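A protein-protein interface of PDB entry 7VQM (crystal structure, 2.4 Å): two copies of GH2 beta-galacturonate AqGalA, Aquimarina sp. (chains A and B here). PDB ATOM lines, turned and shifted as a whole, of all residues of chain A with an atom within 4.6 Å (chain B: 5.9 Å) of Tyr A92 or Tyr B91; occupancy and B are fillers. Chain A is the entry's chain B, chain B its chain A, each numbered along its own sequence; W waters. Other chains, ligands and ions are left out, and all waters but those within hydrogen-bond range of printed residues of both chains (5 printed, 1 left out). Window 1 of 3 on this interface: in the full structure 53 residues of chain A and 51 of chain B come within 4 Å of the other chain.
The backbone carbonyl oxygen (O) of Pro B550 lies within hydrogen-bond range of the side-chain amide nitrogen (ND2) of Asn B553 (3.1 Å).
O of Leu A90 sits at hydrogen-bond distance from ND2 of Asn A83, at 3.1 Å.
The side-chain hydroxyl (OH) of Tyr A92 is in hydrogen-bond range of the backbone carbonyl oxygen (O) of Ser A95 (2.7 Å).
The indole nitrogen of Trp A82 is in hydrogen-bond range of the backbone carbonyl oxygen of Tyr A92.
Ile A24 touches Tyr B91.
Asn B553 touches Ile A24.
Pro A26 touches Tyr B91 (CG to CE1, 3.9 Å).
Pro A26 touches Pro B550 (CG to CB, 3.6 Å).
O of Arg B87 touches CA of Met A88 (3.6 Å).
Met B88 touches Leu A90.
Tyr A91 touches Met B88.
Tyr B91 touches Tyr A92.
Of chain B, only Tyr B91 (3.9 Å) comes within 4 Å of Tyr A92.
Printed residues of chain A within 4 Å of Pro B550: Pro A26 (3.6 Å).
Printed residues of chain A within 4 Å of Met B88: Leu A90 and Tyr A91.
Of the printed residues of chain B, Tyr A91 touches Met B88.
Of the printed residues of chain A, Arg B87 touches Met A88 (3.6 Å).
Printed residues of chain B within 4 Å of Leu A90: Met B88.
Trp A82 touches none of the printed residues of chain B.
The nearest printed residue of chain B that does not touch Tyr A92 is Met B88 (6.2 Å).
The nearest printed residue of chain B that does not touch Met A88 is Tyr B91 (4.003 Å).
Printed residues of chain B that touch a printed residue of chain A: Arg B87, Met B88, Tyr B91, Pro B550 and Asn B553.
Hydrophobic or aromatic side chains of chain B within 4 Å of the printed part of chain A: Met B88, Tyr B91 and Pro B550.
Of the 15 printed residues of chain A, 6 touch a printed residue of chain B.
Printed residues of chain A that touch a printed residue of chain B: Ile A24, Pro A26, Met A88, Leu A90, Tyr A91 and Tyr A92.
Hydrophobic or aromatic side chains of chain A that line the printed part of chain B: Ile A24, Pro A26, Leu A90, Tyr A91 and Tyr A92.
Among the printed residues, no Asp or Glu carboxylate lies within 4 Å of a Lys or Arg side-chain nitrogen of the other chain.
Leu A90 touches Met B88, but with the chains exchanged Met A88 does not touch Leu B90 (4.1 Å).
Tyr A91 touches Met B88, but with the chains exchanged Met A88 does not touch Tyr B91 (4.003 Å).
Tyr A92 touches Tyr B91, but with the chains exchanged Tyr A91 does not touch Tyr B92 (4.1 Å).
Positions printed for both chains: 83, 88, 89, 90, 91, 92 and 93.
Water W1 lies within hydrogen-bond range of the side-chain carboxylate (OD1) of Asp A25 (2.5 Å) and the backbone carbonyl oxygen (O) of Pro B550 (2.7 Å).
Water W5 lies within hydrogen-bond range of the side-chain carboxylate of Glu A93 and the backbone carbonyl oxygen of Glu B93.
Water W2 lies within hydrogen-bond range of the backbone carbonyl oxygen (O) of Ile A24 (2.6 Å), the side-chain hydroxyl (OH) of Tyr B91 (2.9 Å) and the side-chain amide oxygen (OD1) of Asn B553 (3.1 Å).
Water W3 lies within hydrogen-bond range of the backbone carbonyl oxygen of Met B88 (2.7 Å), the backbone NH of Tyr A91 (2.8 Å), the backbone carbonyl oxygen of Met A88 (2.9 Å) and the backbone NH of Leu A90 (3.5 Å).
Water W4 bridges the side-chain carboxylate (OE1) of Glu B93 (2.9 Å) and the backbone carbonyl oxygen (O) of Glu A93 (3.2 Å).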
ATOM      1  N   ILE A  24      17.359 -22.933  26.640  1.00  0.00           N
ATOM      2  CA  ILE A  24      16.492 -21.737  26.488  1.00  0.00           C
ATOM      3  C   ILE A  24      17.071 -20.941  25.314  1.00  0.00           C
ATOM      4  O   ILE A  24      18.274 -20.699  25.338  1.00  0.00           O
ATOM      5  CB  ILE A  24      16.398 -20.933  27.802  1.00  0.00           C
ATOM      6  CG1 ILE A  24      16.360 -21.840  29.039  1.00  0.00           C
ATOM      7  CG2 ILE A  24      15.190 -20.008  27.761  1.00  0.00           C
ATOM      8  CD1 ILE A  24      16.329 -21.100  30.376  1.00  0.00           C
ATOM      9  N   ASP A  25      16.265 -20.606  24.298  1.00  0.00           N
ATOM     10  CA  ASP A  25      16.748 -20.005  23.021  1.00  0.00           C
ATOM     11  C   ASP A  25      15.886 -18.810  22.613  1.00  0.00           C
ATOM     12  O   ASP A  25      15.177 -18.873  21.605  1.00  0.00           O
ATOM     13  CB  ASP A  25      16.757 -21.048  21.899  1.00  0.00           C
ATOM     14  CG  ASP A  25      17.465 -20.590  20.639  1.00  0.00           C
ATOM     15  OD1 ASP A  25      18.195 -19.562  20.707  1.00  0.00           O
ATOM     16  OD2 ASP A  25      17.280 -21.251  19.606  1.00  0.00           O
ATOM     17  N   PRO A  26      15.929 -17.671  23.343  1.00  0.00           N
ATOM     18  CA  PRO A  26      14.961 -16.589  23.117  1.00  0.00           C
ATOM     19  C   PRO A  26      15.058 -15.953  21.711  1.00  0.00           C
ATOM     20  O   PRO A  26      14.047 -15.635  21.118  1.00  0.00           O
ATOM     21  CB  PRO A  26      15.248 -15.583  24.252  1.00  0.00           C
ATOM     22  CG  PRO A  26      16.665 -15.888  24.716  1.00  0.00           C
ATOM     23  CD  PRO A  26      16.898 -17.357  24.403  1.00  0.00           C
ATOM     24  N   TRP A  82       7.218 -25.824  31.651  1.00  0.00           N
ATOM     25  CA  TRP A  82       8.551 -25.361  32.101  1.00  0.00           C
ATOM     26  C   TRP A  82       8.401 -24.363  33.260  1.00  0.00           C
ATOM     27  O   TRP A  82       9.250 -24.388  34.171  1.00  0.00           O
ATOM     28  CB  TRP A  82       9.394 -24.840  30.927  1.00  0.00           C
ATOM     29  CG  TRP A  82       8.890 -23.686  30.121  1.00  0.00           C
ATOM     30  CD1 TRP A  82       8.551 -22.444  30.564  1.00  0.00           C
ATOM     31  CD2 TRP A  82       8.803 -23.626  28.688  1.00  0.00           C
ATOM     32  NE1 TRP A  82       8.213 -21.634  29.514  1.00  0.00           N
ATOM     33  CE2 TRP A  82       8.373 -22.327  28.349  1.00  0.00           C
ATOM     34  CE3 TRP A  82       9.035 -24.543  27.660  1.00  0.00           C
ATOM     35  CZ2 TRP A  82       8.165 -21.929  27.033  1.00  0.00           C
ATOM     36  CZ3 TRP A  82       8.848 -24.142  26.358  1.00  0.00           C
ATOM     37  CH2 TRP A  82       8.401 -22.862  26.047  1.00  0.00           C
ATOM     38  N   ASN A  83       7.318 -23.589  33.280  1.00  0.00           N
ATOM     39  CA  ASN A  83       7.156 -22.397  34.154  1.00  0.00           C
ATOM     40  C   ASN A  83       7.289 -22.767  35.643  1.00  0.00           C
ATOM     41  O   ASN A  83       7.895 -21.994  36.412  1.00  0.00           O
ATOM     42  CB  ASN A  83       5.802 -21.732  33.912  1.00  0.00           C
ATOM     43  CG  ASN A  83       5.529 -21.484  32.445  1.00  0.00           C
ATOM     44  OD1 ASN A  83       5.425 -22.420  31.654  1.00  0.00           O
ATOM     45  ND2 ASN A  83       5.421 -20.220  32.083  1.00  0.00           N
ATOM     46  N   MET A  88      13.268 -19.111  37.079  1.00  0.00           N
ATOM     47  CA  MET A  88      13.847 -18.608  35.813  1.00  0.00           C
ATOM     48  C   MET A  88      12.803 -18.727  34.699  1.00  0.00           C
ATOM     49  O   MET A  88      12.822 -17.883  33.800  1.00  0.00           O
ATOM     50  CB  MET A  88      15.091 -19.427  35.438  1.00  0.00           C
ATOM     51  CG  MET A  88      15.930 -18.799  34.371  1.00  0.00           C
ATOM     52  SD  MET A  88      17.526 -19.609  34.177  1.00  0.00           S
ATOM     53  CE  MET A  88      16.999 -21.317  34.048  1.00  0.00           C
ATOM     54  N   LEU A  89      11.972 -19.769  34.726  1.00  0.00           N
ATOM     55  CA  LEU A  89      11.070 -20.088  33.590  1.00  0.00           C
ATOM     56  C   LEU A  89       9.643 -19.633  33.897  1.00  0.00           C
ATOM     57  O   LEU A  89       8.811 -19.713  32.989  1.00  0.00           O
ATOM     58  CB  LEU A  89      11.140 -21.591  33.301  1.00  0.00           C
ATOM     59  CG  LEU A  89      12.486 -22.080  32.777  1.00  0.00           C
ATOM     60  CD1 LEU A  89      12.690 -23.553  33.052  1.00  0.00           C
ATOM     61  CD2 LEU A  89      12.623 -21.802  31.288  1.00  0.00           C
ATOM     62  N   LEU A  90       9.376 -19.152  35.106  1.00  0.00           N
ATOM     63  CA  LEU A  90       8.019 -18.717  35.538  1.00  0.00           C
ATOM     64  C   LEU A  90       7.388 -17.782  34.494  1.00  0.00           C
ATOM     65  O   LEU A  90       6.232 -18.022  34.108  1.00  0.00           O
ATOM     66  CB  LEU A  90       8.129 -18.026  36.900  1.00  0.00           C
ATOM     67  CG  LEU A  90       6.833 -17.430  37.450  1.00  0.00           C
ATOM     68  CD1 LEU A  90       5.786 -18.513  37.656  1.00  0.00           C
ATOM     69  CD2 LEU A  90       7.104 -16.674  38.744  1.00  0.00           C
ATOM     70  N   TYR A  91       8.123 -16.777  34.019  1.00  0.00           N
ATOM     71  CA  TYR A  91       7.617 -15.773  33.056  1.00  0.00           C
ATOM     72  C   TYR A  91       8.171 -16.026  31.635  1.00  0.00           C
ATOM     73  O   TYR A  91       7.842 -15.227  30.715  1.00  0.00           O
ATOM     74  CB  TYR A  91       7.907 -14.381  33.618  1.00  0.00           C
ATOM     75  CG  TYR A  91       6.903 -13.869  34.634  1.00  0.00           C
ATOM     76  CD1 TYR A  91       5.706 -13.307  34.208  1.00  0.00           C
ATOM     77  CD2 TYR A  91       7.140 -13.900  36.008  1.00  0.00           C
ATOM     78  CE1 TYR A  91       4.779 -12.794  35.103  1.00  0.00           C
ATOM     79  CE2 TYR A  91       6.215 -13.398  36.918  1.00  0.00           C
ATOM     80  CZ  TYR A  91       5.026 -12.840  36.464  1.00  0.00           C
ATOM     81  OH  TYR A  91       4.073 -12.320  37.298  1.00  0.00           O
ATOM     82  N   TYR A  92       8.912 -17.117  31.391  1.00  0.00           N
ATOM     83  CA  TYR A  92       9.520 -17.363  30.050  1.00  0.00           C
ATOM     84  C   TYR A  92       8.410 -17.590  29.010  1.00  0.00           C
ATOM     85  O   TYR A  92       7.644 -18.545  29.080  1.00  0.00           O
ATOM     86  CB  TYR A  92      10.534 -18.517  30.006  1.00  0.00           C
ATOM     87  CG  TYR A  92      11.269 -18.592  28.688  1.00  0.00           C
ATOM     88  CD1 TYR A  92      12.136 -17.583  28.301  1.00  0.00           C
ATOM     89  CD2 TYR A  92      11.064 -19.625  27.792  1.00  0.00           C
ATOM     90  CE1 TYR A  92      12.791 -17.608  27.079  1.00  0.00           C
ATOM     91  CE2 TYR A  92      11.711 -19.671  26.565  1.00  0.00           C
ATOM     92  CZ  TYR A  92      12.581 -18.658  26.201  1.00  0.00           C
ATOM     93  OH  TYR A  92      13.240 -18.678  25.001  1.00  0.00           O
ATOM     94  N   GLU A  93       8.338 -16.686  28.038  1.00  0.00           N
ATOM     95  CA  GLU A  93       7.463 -16.783  26.846  1.00  0.00           C
ATOM     96  C   GLU A  93       8.402 -16.719  25.635  1.00  0.00           C
ATOM     97  O   GLU A  93       9.076 -15.695  25.468  1.00  0.00           O
ATOM     98  CB  GLU A  93       6.394 -15.690  26.894  1.00  0.00           C
ATOM     99  CG  GLU A  93       5.803 -15.388  25.528  1.00  0.00           C
ATOM    100  CD  GLU A  93       5.176 -14.010  25.365  1.00  0.00           C
ATOM    101  OE1 GLU A  93       4.853 -13.379  26.427  1.00  0.00           O
ATOM    102  OE2 GLU A  93       4.986 -13.583  24.187  1.00  0.00           O
ATOM    103  N   GLY A  94       8.512 -17.804  24.875  1.00  0.00           N
ATOM    104  CA  GLY A  94       9.596 -17.972  23.891  1.00  0.00           C
ATOM    105  C   GLY A  94       9.826 -19.432  23.544  1.00  0.00           C
ATOM    106  O   GLY A  94       8.903 -20.259  23.809  1.00  0.00           O
ATOM    107  N   SER A  95      11.001 -19.729  22.970  1.00  0.00           N
ATOM    108  CA  SER A  95      11.354 -21.056  22.410  1.00  0.00           C
ATOM    109  C   SER A  95      12.366 -21.769  23.316  1.00  0.00           C
ATOM    110  O   SER A  95      13.304 -21.123  23.858  1.00  0.00           O
ATOM    111  CB  SER A  95      11.841 -20.948  20.986  1.00  0.00           C
ATOM    112  OG  SER A  95      13.216 -20.594  20.920  1.00  0.00           O
ATOM    113  N   LEU A  96      12.198 -23.077  23.444  1.00  0.00           N
ATOM    114  CA  LEU A  96      13.058 -23.940  24.280  1.00  0.00           C
ATOM    115  C   LEU A  96      13.258 -25.276  23.554  1.00  0.00           C
ATOM    116  O   LEU A  96      12.279 -25.797  22.973  1.00  0.00           O
ATOM    117  CB  LEU A  96      12.342 -24.072  25.624  1.00  0.00           C
ATOM    118  CG  LEU A  96      13.115 -24.779  26.722  1.00  0.00           C
ATOM    119  CD1 LEU A  96      12.832 -24.133  28.053  1.00  0.00           C
ATOM    120  CD2 LEU A  96      12.771 -26.257  26.765  1.00  0.00           C
ATOM    121  N   ASN A 163       6.171 -20.807  22.673  1.00  0.00           N
ATOM    122  CA  ASN A 163       4.898 -20.351  23.279  1.00  0.00           C
ATOM    123  C   ASN A 163       4.815 -18.827  23.173  1.00  0.00           C
ATOM    124  O   ASN A 163       3.972 -18.241  23.865  1.00  0.00           O
ATOM    125  CB  ASN A 163       4.752 -20.889  24.706  1.00  0.00           C
ATOM    126  CG  ASN A 163       5.485 -20.068  25.748  1.00  0.00           C
ATOM    127  OD1 ASN A 163       6.475 -19.408  25.449  1.00  0.00           O
ATOM    128  ND2 ASN A 163       4.989 -20.101  26.975  1.00  0.00           N
ATOM    129  N   ASN B  83      16.844  -7.552  34.783  1.00  0.00           N
ATOM    130  CA  ASN B  83      17.206  -8.984  34.575  1.00  0.00           C
ATOM    131  C   ASN B  83      18.124  -9.491  35.685  1.00  0.00           C
ATOM    132  O   ASN B  83      18.005 -10.694  36.007  1.00  0.00           O
ATOM    133  CB  ASN B  83      17.922  -9.254  33.247  1.00  0.00           C
ATOM    134  CG  ASN B  83      17.202  -8.631  32.080  1.00  0.00           C
ATOM    135  OD1 ASN B  83      17.199  -7.413  31.960  1.00  0.00           O
ATOM    136  ND2 ASN B  83      16.565  -9.448  31.256  1.00  0.00           N
ATOM    137  N   ARG B  87      16.385 -13.803  39.605  1.00  0.00           N
ATOM    138  CA  ARG B  87      16.315 -14.987  38.698  1.00  0.00           C
ATOM    139  C   ARG B  87      15.023 -14.968  37.851  1.00  0.00           C
ATOM    140  O   ARG B  87      15.093 -15.293  36.656  1.00  0.00           O
ATOM    141  CB  ARG B  87      16.368 -16.258  39.546  1.00  0.00           C
ATOM    142  CG  ARG B  87      16.577 -17.547  38.764  1.00  0.00           C
ATOM    143  CD  ARG B  87      16.710 -18.668  39.783  1.00  0.00           C
ATOM    144  NE  ARG B  87      16.942 -19.990  39.226  1.00  0.00           N
ATOM    145  CZ  ARG B  87      18.097 -20.407  38.708  1.00  0.00           C
ATOM    146  NH1 ARG B  87      19.125 -19.578  38.626  1.00  0.00           N
ATOM    147  NH2 ARG B  87      18.210 -21.642  38.249  1.00  0.00           N
ATOM    148  N   MET B  88      13.882 -14.614  38.461  1.00  0.00           N
ATOM    149  CA  MET B  88      12.557 -14.488  37.792  1.00  0.00           C
ATOM    150  C   MET B  88      12.610 -13.530  36.579  1.00  0.00           C
ATOM    151  O   MET B  88      11.845 -13.758  35.639  1.00  0.00           O
ATOM    152  CB  MET B  88      11.526 -13.977  38.800  1.00  0.00           C
ATOM    153  CG  MET B  88      10.115 -13.971  38.283  1.00  0.00           C
ATOM    154  SD  MET B  88       8.972 -13.558  39.600  1.00  0.00           S
ATOM    155  CE  MET B  88       9.518 -11.894  39.991  1.00  0.00           C
ATOM    156  N   LEU B  89      13.456 -12.491  36.613  1.00  0.00           N
ATOM    157  CA  LEU B  89      13.494 -11.385  35.612  1.00  0.00           C
ATOM    158  C   LEU B  89      14.598 -11.605  34.561  1.00  0.00           C
ATOM    159  O   LEU B  89      14.662 -10.822  33.595  1.00  0.00           O
ATOM    160  CB  LEU B  89      13.667 -10.063  36.375  1.00  0.00           C
ATOM    161  CG  LEU B  89      12.451  -9.632  37.211  1.00  0.00           C
ATOM    162  CD1 LEU B  89      12.681  -8.289  37.895  1.00  0.00           C
ATOM    163  CD2 LEU B  89      11.177  -9.566  36.370  1.00  0.00           C
ATOM    164  N   LEU B  90      15.401 -12.657  34.690  1.00  0.00           N
ATOM    165  CA  LEU B  90      16.615 -12.850  33.858  1.00  0.00           C
ATOM    166  C   LEU B  90      16.243 -12.921  32.371  1.00  0.00           C
ATOM    167  O   LEU B  90      16.883 -12.228  31.558  1.00  0.00           O
ATOM    168  CB  LEU B  90      17.350 -14.112  34.303  1.00  0.00           C
ATOM    169  CG  LEU B  90      18.622 -14.405  33.511  1.00  0.00           C
ATOM    170  CD1 LEU B  90      19.728 -13.416  33.868  1.00  0.00           C
ATOM    171  CD2 LEU B  90      19.082 -15.841  33.738  1.00  0.00           C
ATOM    172  N   TYR B  91      15.229 -13.701  32.010  1.00  0.00           N
ATOM    173  CA  TYR B  91      14.782 -13.826  30.603  1.00  0.00           C
ATOM    174  C   TYR B  91      13.498 -13.031  30.357  1.00  0.00           C
ATOM    175  O   TYR B  91      12.980 -13.182  29.246  1.00  0.00           O
ATOM    176  CB  TYR B  91      14.597 -15.296  30.239  1.00  0.00           C
ATOM    177  CG  TYR B  91      15.880 -16.040  29.967  1.00  0.00           C
ATOM    178  CD1 TYR B  91      16.480 -15.983  28.725  1.00  0.00           C
ATOM    179  CD2 TYR B  91      16.487 -16.810  30.942  1.00  0.00           C
ATOM    180  CE1 TYR B  91      17.654 -16.667  28.456  1.00  0.00           C
ATOM    181  CE2 TYR B  91      17.654 -17.515  30.687  1.00  0.00           C
ATOM    182  CZ  TYR B  91      18.242 -17.449  29.435  1.00  0.00           C
ATOM    183  OH  TYR B  91      19.386 -18.149  29.146  1.00  0.00           O
ATOM    184  N   TYR B  92      13.025 -12.201  31.298  1.00  0.00           N
ATOM    185  CA  TYR B  92      11.768 -11.434  31.106  1.00  0.00           C
ATOM    186  C   TYR B  92      11.936 -10.409  29.985  1.00  0.00           C
ATOM    187  O   TYR B  92      12.756  -9.472  30.081  1.00  0.00           O
ATOM    188  CB  TYR B  92      11.261 -10.682  32.333  1.00  0.00           C
ATOM    189  CG  TYR B  92       9.912 -10.053  32.069  1.00  0.00           C
ATOM    190  CD1 TYR B  92       8.821 -10.855  31.819  1.00  0.00           C
ATOM    191  CD2 TYR B  92       9.724  -8.681  31.991  1.00  0.00           C
ATOM    192  CE1 TYR B  92       7.579 -10.328  31.520  1.00  0.00           C
ATOM    193  CE2 TYR B  92       8.479  -8.129  31.715  1.00  0.00           C
ATOM    194  CZ  TYR B  92       7.399  -8.963  31.477  1.00  0.00           C
ATOM    195  OH  TYR B  92       6.139  -8.517  31.211  1.00  0.00           O
ATOM    196  N   GLU B  93      11.110 -10.585  28.958  1.00  0.00           N
ATOM    197  CA  GLU B  93      11.023  -9.725  27.753  1.00  0.00           C
ATOM    198  C   GLU B  93       9.562  -9.282  27.624  1.00  0.00           C
ATOM    199  O   GLU B  93       8.715 -10.142  27.294  1.00  0.00           O
ATOM    200  CB  GLU B  93      11.494 -10.522  26.533  1.00  0.00           C
ATOM    201  CG  GLU B  93      10.982  -9.938  25.234  1.00  0.00           C
ATOM    202  CD  GLU B  93      11.305 -10.723  23.982  1.00  0.00           C
ATOM    203  OE1 GLU B  93      12.140 -11.659  24.084  1.00  0.00           O
ATOM    204  OE2 GLU B  93      10.721 -10.390  22.916  1.00  0.00           O
ATOM    205  N   TRP B 178      22.490  -9.471  25.576  1.00  0.00           N
ATOM    206  CA  TRP B 178      21.317  -9.741  26.456  1.00  0.00           C
ATOM    207  C   TRP B 178      20.332  -8.572  26.405  1.00  0.00           C
ATOM    208  O   TRP B 178      20.795  -7.436  26.524  1.00  0.00           O
ATOM    209  CB  TRP B 178      21.776  -9.975  27.892  1.00  0.00           C
ATOM    210  CG  TRP B 178      20.900 -10.934  28.619  1.00  0.00           C
ATOM    211  CD1 TRP B 178      19.810 -10.676  29.401  1.00  0.00           C
ATOM    212  CD2 TRP B 178      21.043 -12.357  28.578  1.00  0.00           C
ATOM    213  NE1 TRP B 178      19.279 -11.852  29.865  1.00  0.00           N
ATOM    214  CE2 TRP B 178      20.023 -12.896  29.380  1.00  0.00           C
ATOM    215  CE3 TRP B 178      21.957 -13.211  27.959  1.00  0.00           C
ATOM    216  CZ2 TRP B 178      19.888 -14.265  29.561  1.00  0.00           C
ATOM    217  CZ3 TRP B 178      21.834 -14.563  28.159  1.00  0.00           C
ATOM    218  CH2 TRP B 178      20.807 -15.080  28.942  1.00  0.00           C
ATOM    219  N   ARG B 548      27.427 -10.946  28.348  1.00  0.00           N
ATOM    220  CA  ARG B 548      26.295 -11.890  28.320  1.00  0.00           C
ATOM    221  C   ARG B 548      25.652 -11.851  26.931  1.00  0.00           C
ATOM    222  O   ARG B 548      25.482 -10.724  26.390  1.00  0.00           O
ATOM    223  CB  ARG B 548      25.329 -11.529  29.451  1.00  0.00           C
ATOM    224  CG  ARG B 548      25.943 -11.685  30.835  1.00  0.00           C
ATOM    225  CD  ARG B 548      26.095 -13.151  31.221  1.00  0.00           C
ATOM    226  NE  ARG B 548      24.801 -13.837  31.261  1.00  0.00           N
ATOM    227  CZ  ARG B 548      24.619 -15.152  31.353  1.00  0.00           C
ATOM    228  NH1 ARG B 548      25.647 -15.973  31.450  1.00  0.00           N
ATOM    229  NH2 ARG B 548      23.394 -15.636  31.358  1.00  0.00           N
ATOM    230  N   PRO B 550      22.425 -14.417  24.908  1.00  0.00           N
ATOM    231  CA  PRO B 550      21.595 -15.616  24.822  1.00  0.00           C
ATOM    232  C   PRO B 550      21.750 -16.358  23.484  1.00  0.00           C
ATOM    233  O   PRO B 550      21.000 -17.296  23.266  1.00  0.00           O
ATOM    234  CB  PRO B 550      20.175 -15.045  24.957  1.00  0.00           C
ATOM    235  CG  PRO B 550      20.284 -13.712  24.264  1.00  0.00           C
ATOM    236  CD  PRO B 550      21.634 -13.188  24.710  1.00  0.00           C
ATOM    237  N   ASN B 553      25.361 -20.603  23.857  1.00  0.00           N
ATOM    238  CA  ASN B 553      24.571 -21.596  24.632  1.00  0.00           C
ATOM    239  C   ASN B 553      25.376 -22.877  24.823  1.00  0.00           C
ATOM    240  O   ASN B 553      24.769 -23.895  25.141  1.00  0.00           O
ATOM    241  CB  ASN B 553      23.225 -21.847  23.949  1.00  0.00           C
ATOM    242  CG  ASN B 553      22.263 -20.707  24.212  1.00  0.00           C
ATOM    243  OD1 ASN B 553      22.275 -20.114  25.291  1.00  0.00           O
ATOM    244  ND2 ASN B 553      21.477 -20.352  23.216  1.00  0.00           N
HETATM  245  O   HOH W   1      18.896 -17.286  21.524  1.00  0.00           O
HETATM  246  O   HOH W   2      19.734 -18.703  26.284  1.00  0.00           O
HETATM  247  O   HOH W   3      10.791 -16.007  34.514  1.00  0.00           O
HETATM  248  O   HOH W   4      11.949 -14.524  24.699  1.00  0.00           O
HETATM  249  O   HOH W   5       6.060 -11.894  28.142  1.00  0.00           O
